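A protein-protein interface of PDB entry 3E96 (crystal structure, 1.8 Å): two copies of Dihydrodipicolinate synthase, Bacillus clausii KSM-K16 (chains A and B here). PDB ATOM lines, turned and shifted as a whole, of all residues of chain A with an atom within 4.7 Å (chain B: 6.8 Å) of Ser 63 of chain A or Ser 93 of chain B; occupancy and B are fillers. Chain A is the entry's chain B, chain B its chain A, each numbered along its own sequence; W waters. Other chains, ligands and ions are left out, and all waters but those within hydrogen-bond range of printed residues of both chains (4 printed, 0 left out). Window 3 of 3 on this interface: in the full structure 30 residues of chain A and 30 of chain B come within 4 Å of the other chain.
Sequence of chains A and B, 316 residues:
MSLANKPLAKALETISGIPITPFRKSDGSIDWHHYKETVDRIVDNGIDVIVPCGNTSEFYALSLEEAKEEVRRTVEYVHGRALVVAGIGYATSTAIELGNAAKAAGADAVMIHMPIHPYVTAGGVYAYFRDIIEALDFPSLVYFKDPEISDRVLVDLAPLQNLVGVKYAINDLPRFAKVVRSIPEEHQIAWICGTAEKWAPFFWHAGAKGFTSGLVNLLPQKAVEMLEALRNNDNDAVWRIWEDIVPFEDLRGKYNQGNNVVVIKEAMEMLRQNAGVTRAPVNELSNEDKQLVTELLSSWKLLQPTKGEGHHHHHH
The side-chain carboxylate of Glu 66 of chain A lies within hydrogen-bond range of the backbone NH of Ser 63 of chain A, at 3.0 Å.
Ala 61 of chain A touches Ala 91 of chain B. Ala 91 of chain B touches Leu 62 of chain A (CB to O, 3.6 Å). CB of Ser 63 of chain A touches OG of Ser 93 of chain B, at 3.5 Å. Ser 63 of chain A touches Thr 94 of chain B (CA to OG1, 3.9 Å).
Of the printed residues of chain B, Ala 61 of chain A touches Ala 91. Ser 63 of chain A touches just these residues of chain B: Ser 93 and Thr 94. Printed residues of chain A within 4 Å of Ala 91 of chain B: Ala 61 and Leu 62. Of chain A, only Ser 63 (3.5 Å) comes within 4 Å of Ser 93 of chain B. Of the printed residues of chain A, Thr 94 of chain B touches Ser 63.
Hydrophobic or aromatic side chains of chain B within 4 Å of the printed part of chain A: Ala 91. Of the 7 printed residues of chain A, 3 touch a printed residue of chain B. Among the printed residues, no Asp or Glu carboxylate lies within 4 Å of a Lys or Arg side-chain nitrogen of the other chain.
No position is printed for both chains. Of the 4 pairs that touch across the chains among the printed residues, none has its exchanged pair printed and touching as well.
Water W2 bridges the side-chain hydroxyl of Thr 94 of chain B and the backbone NH of Leu 64 of chain A. Water W4 bridges O of Ala 61 of chain A (2.7 Å) and N of Thr 92 of chain B (3.2 Å). Water W3 lies within hydrogen-bond range of the side-chain carboxylate (OE1) of Glu 66 of chain A (2.7 Å) and the side-chain hydroxyl (OG) of Ser 93 of chain B (2.9 Å). Water W1 lies within hydrogen-bond range of O of Leu 62 of chain A, N of Ala 91 of chain B and OG1 of Thr 94 of chain B.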
ATOM      1  N   ALA A  61       6.075 -22.023   6.285  1.00  0.00           N
ATOM      2  CA  ALA A  61       7.248 -22.809   5.893  1.00  0.00           C
ATOM      3  C   ALA A  61       8.287 -21.888   5.246  1.00  0.00           C
ATOM      4  O   ALA A  61       9.367 -22.329   4.844  1.00  0.00           O
ATOM      5  CB  ALA A  61       6.838 -23.907   4.918  1.00  0.00           C
ATOM      6  N   LEU A  62       7.956 -20.603   5.149  1.00  0.00           N
ATOM      7  CA  LEU A  62       8.864 -19.622   4.555  1.00  0.00           C
ATOM      8  C   LEU A  62       9.600 -18.828   5.626  1.00  0.00           C
ATOM      9  O   LEU A  62       9.067 -18.583   6.706  1.00  0.00           O
ATOM     10  CB  LEU A  62       8.084 -18.625   3.688  1.00  0.00           C
ATOM     11  CG  LEU A  62       7.148 -19.132   2.587  1.00  0.00           C
ATOM     12  CD1 LEU A  62       6.397 -17.943   1.991  1.00  0.00           C
ATOM     13  CD2 LEU A  62       7.942 -19.861   1.515  1.00  0.00           C
ATOM     14  N   SER A  63      10.831 -18.427   5.330  1.00  0.00           N
ATOM     15  CA  SER A  63      11.574 -17.604   6.276  1.00  0.00           C
ATOM     16  C   SER A  63      10.944 -16.222   6.106  1.00  0.00           C
ATOM     17  O   SER A  63      10.198 -15.995   5.148  1.00  0.00           O
ATOM     18  CB  SER A  63      13.050 -17.543   5.895  1.00  0.00           C
ATOM     19  OG  SER A  63      13.212 -16.883   4.653  1.00  0.00           O
ATOM     20  N   LEU A  64      11.224 -15.304   7.023  1.00  0.00           N
ATOM     21  CA  LEU A  64      10.663 -13.960   6.919  1.00  0.00           C
ATOM     22  C   LEU A  64      11.100 -13.296   5.620  1.00  0.00           C
ATOM     23  O   LEU A  64      10.322 -12.588   4.981  1.00  0.00           O
ATOM     24  CB  LEU A  64      11.104 -13.095   8.103  1.00  0.00           C
ATOM     25  CG  LEU A  64      10.527 -13.434   9.478  1.00  0.00           C
ATOM     26  CD1 LEU A  64      11.025 -12.408  10.502  1.00  0.00           C
ATOM     27  CD2 LEU A  64       8.996 -13.420   9.412  1.00  0.00           C
ATOM     28  N   GLU A  65      12.350 -13.525   5.231  1.00  0.00           N
ATOM     29  CA  GLU A  65      12.873 -12.937   4.004  1.00  0.00           C
ATOM     30  C   GLU A  65      12.199 -13.536   2.768  1.00  0.00           C
ATOM     31  O   GLU A  65      11.935 -12.829   1.797  1.00  0.00           O
ATOM     32  CB  GLU A  65      14.396 -13.133   3.940  1.00  0.00           C
ATOM     33  CG  GLU A  65      15.074 -12.532   2.711  1.00  0.00           C
ATOM     34  CD  GLU A  65      14.742 -11.060   2.507  1.00  0.00           C
ATOM     35  OE1 GLU A  65      14.699 -10.306   3.504  1.00  0.00           O
ATOM     36  OE2 GLU A  65      14.535 -10.658   1.341  1.00  0.00           O
ATOM     37  N   GLU A  66      11.925 -14.838   2.795  1.00  0.00           N
ATOM     38  CA  GLU A  66      11.263 -15.474   1.663  1.00  0.00           C
ATOM     39  C   GLU A  66       9.831 -14.962   1.540  1.00  0.00           C
ATOM     40  O   GLU A  66       9.310 -14.809   0.432  1.00  0.00           O
ATOM     41  CB  GLU A  66      11.244 -16.994   1.824  1.00  0.00           C
ATOM     42  CG  GLU A  66      12.582 -17.665   1.613  1.00  0.00           C
ATOM     43  CD  GLU A  66      12.487 -19.168   1.780  1.00  0.00           C
ATOM     44  OE1 GLU A  66      11.893 -19.615   2.782  1.00  0.00           O
ATOM     45  OE2 GLU A  66      13.006 -19.903   0.916  1.00  0.00           O
ATOM     46  N   ALA A  67       9.192 -14.702   2.679  1.00  0.00           N
ATOM     47  CA  ALA A  67       7.823 -14.194   2.677  1.00  0.00           C
ATOM     48  C   ALA A  67       7.802 -12.809   2.031  1.00  0.00           C
ATOM     49  O   ALA A  67       6.949 -12.518   1.195  1.00  0.00           O
ATOM     50  CB  ALA A  67       7.284 -14.114   4.100  1.00  0.00           C
ATOM     51  N   GLY B  89      11.915 -22.572  16.798  1.00  0.00           N
ATOM     52  CA  GLY B  89      10.799 -23.000  15.976  1.00  0.00           C
ATOM     53  C   GLY B  89      10.743 -22.279  14.642  1.00  0.00           C
ATOM     54  O   GLY B  89      11.756 -21.756  14.174  1.00  0.00           O
ATOM     55  N   TYR B  90       9.549 -22.260  14.048  1.00  0.00           N
ATOM     56  CA  TYR B  90       9.274 -21.624  12.760  1.00  0.00           C
ATOM     57  C   TYR B  90       9.800 -22.449  11.591  1.00  0.00           C
ATOM     58  O   TYR B  90      10.075 -23.643  11.737  1.00  0.00           O
ATOM     59  CB  TYR B  90       9.863 -20.211  12.726  1.00  0.00           C
ATOM     60  CG  TYR B  90       9.329 -19.307  13.819  1.00  0.00           C
ATOM     61  CD1 TYR B  90       7.967 -18.993  13.893  1.00  0.00           C
ATOM     62  CD2 TYR B  90      10.185 -18.757  14.774  1.00  0.00           C
ATOM     63  CE1 TYR B  90       7.477 -18.146  14.893  1.00  0.00           C
ATOM     64  CE2 TYR B  90       9.706 -17.914  15.771  1.00  0.00           C
ATOM     65  CZ  TYR B  90       8.356 -17.612  15.825  1.00  0.00           C
ATOM     66  OH  TYR B  90       7.889 -16.769  16.807  1.00  0.00           O
ATOM     67  N   ALA B  91       9.910 -21.821  10.424  1.00  0.00           N
ATOM     68  CA  ALA B  91      10.406 -22.513   9.241  1.00  0.00           C
ATOM     69  C   ALA B  91      11.784 -23.099   9.526  1.00  0.00           C
ATOM     70  O   ALA B  91      12.555 -22.549  10.310  1.00  0.00           O
ATOM     71  CB  ALA B  91      10.482 -21.549   8.058  1.00  0.00           C
ATOM     72  N   THR B  92      12.080 -24.219   8.875  1.00  0.00           N
ATOM     73  CA  THR B  92      13.349 -24.913   9.041  1.00  0.00           C
ATOM     74  C   THR B  92      14.563 -23.990   9.097  1.00  0.00           C
ATOM     75  O   THR B  92      15.333 -24.033  10.054  1.00  0.00           O
ATOM     76  CB  THR B  92      13.553 -25.930   7.902  1.00  0.00           C
ATOM     77  OG1 THR B  92      12.479 -26.877   7.931  1.00  0.00           O
ATOM     78  CG2 THR B  92      14.876 -26.659   8.062  1.00  0.00           C
ATOM     79  N   SER B  93      14.736 -23.154   8.078  1.00  0.00           N
ATOM     80  CA  SER B  93      15.883 -22.252   8.050  1.00  0.00           C
ATOM     81  C   SER B  93      15.908 -21.322   9.259  1.00  0.00           C
ATOM     82  O   SER B  93      16.978 -20.997   9.780  1.00  0.00           O
ATOM     83  CB  SER B  93      15.884 -21.422   6.757  1.00  0.00           C
ATOM     84  OG  SER B  93      14.790 -20.521   6.722  1.00  0.00           O
ATOM     85  N   THR B  94      14.730 -20.891   9.698  1.00  0.00           N
ATOM     86  CA  THR B  94      14.621 -19.996  10.846  1.00  0.00           C
ATOM     87  C   THR B  94      14.942 -20.739  12.142  1.00  0.00           C
ATOM     88  O   THR B  94      15.630 -20.207  13.015  1.00  0.00           O
ATOM     89  CB  THR B  94      13.204 -19.387  10.938  1.00  0.00           C
ATOM     90  OG1 THR B  94      12.919 -18.675   9.726  1.00  0.00           O
ATOM     91  CG2 THR B  94      13.105 -18.415  12.115  1.00  0.00           C
ATOM     92  N   ALA B  95      14.450 -21.970  12.263  1.00  0.00           N
ATOM     93  CA  ALA B  95      14.714 -22.769  13.457  1.00  0.00           C
ATOM     94  C   ALA B  95      16.224 -22.991  13.568  1.00  0.00           C
ATOM     95  O   ALA B  95      16.796 -22.935  14.651  1.00  0.00           O
ATOM     96  CB  ALA B  95      13.989 -24.113  13.369  1.00  0.00           C
ATOM     97  N   ILE B  96      16.868 -23.236  12.434  1.00  0.00           N
ATOM     98  CA  ILE B  96      18.309 -23.452  12.432  1.00  0.00           C
ATOM     99  C   ILE B  96      19.048 -22.168  12.817  1.00  0.00           C
ATOM    100  O   ILE B  96      20.042 -22.205  13.542  1.00  0.00           O
ATOM    101  CB  ILE B  96      18.775 -23.968  11.057  1.00  0.00           C
ATOM    102  CG1 ILE B  96      18.232 -25.386  10.846  1.00  0.00           C
ATOM    103  CG2 ILE B  96      20.302 -23.957  10.973  1.00  0.00           C
ATOM    104  CD1 ILE B  96      18.385 -25.909   9.429  1.00  0.00           C
ATOM    105  N   GLU B  97      18.553 -21.027  12.346  1.00  0.00           N
ATOM    106  CA  GLU B  97      19.173 -19.748  12.678  1.00  0.00           C
ATOM    107  C   GLU B  97      19.083 -19.528  14.191  1.00  0.00           C
ATOM    108  O   GLU B  97      20.052 -19.125  14.827  1.00  0.00           O
ATOM    109  CB  GLU B  97      18.461 -18.612  11.945  1.00  0.00           C
ATOM    110  CG  GLU B  97      19.041 -17.229  12.213  1.00  0.00           C
ATOM    111  CD  GLU B  97      18.233 -16.138  11.541  1.00  0.00           C
ATOM    112  OE1 GLU B  97      17.866 -16.317  10.361  1.00  0.00           O
ATOM    113  OE2 GLU B  97      17.964 -15.102  12.182  1.00  0.00           O
ATOM    114  N   LEU B  98      17.911 -19.792  14.760  1.00  0.00           N
ATOM    115  CA  LEU B  98      17.713 -19.635  16.200  1.00  0.00           C
ATOM    116  C   LEU B  98      18.600 -20.611  16.972  1.00  0.00           C
ATOM    117  O   LEU B  98      19.132 -20.275  18.029  1.00  0.00           O
ATOM    118  CB  LEU B  98      16.245 -19.885  16.568  1.00  0.00           C
ATOM    119  CG  LEU B  98      15.263 -18.780  16.185  1.00  0.00           C
ATOM    120  CD1 LEU B  98      13.829 -19.259  16.401  1.00  0.00           C
ATOM    121  CD2 LEU B  98      15.554 -17.540  17.022  1.00  0.00           C
ATOM    122  N   ILE B 132      16.119 -30.386  11.181  1.00  0.00           N
ATOM    123  CA  ILE B 132      16.630 -29.352  12.066  1.00  0.00           C
ATOM    124  C   ILE B 132      17.695 -29.931  12.991  1.00  0.00           C
ATOM    125  O   ILE B 132      18.754 -29.328  13.194  1.00  0.00           O
ATOM    126  CB  ILE B 132      15.490 -28.728  12.901  1.00  0.00           C
ATOM    127  CG1 ILE B 132      14.533 -27.972  11.971  1.00  0.00           C
ATOM    128  CG2 ILE B 132      16.068 -27.792  13.962  1.00  0.00           C
ATOM    129  CD1 ILE B 132      13.212 -27.561  12.625  1.00  0.00           C
HETATM  130  O   HOH W   1       9.609 -18.748   9.596  1.00  0.00           O
HETATM  131  O   HOH W   2      12.803 -16.081   9.382  1.00  0.00           O
HETATM  132  O   HOH W   3      13.760 -21.076   4.088  1.00  0.00           O
HETATM  133  O   HOH W   4      10.543 -24.380   6.118  1.00  0.00           O
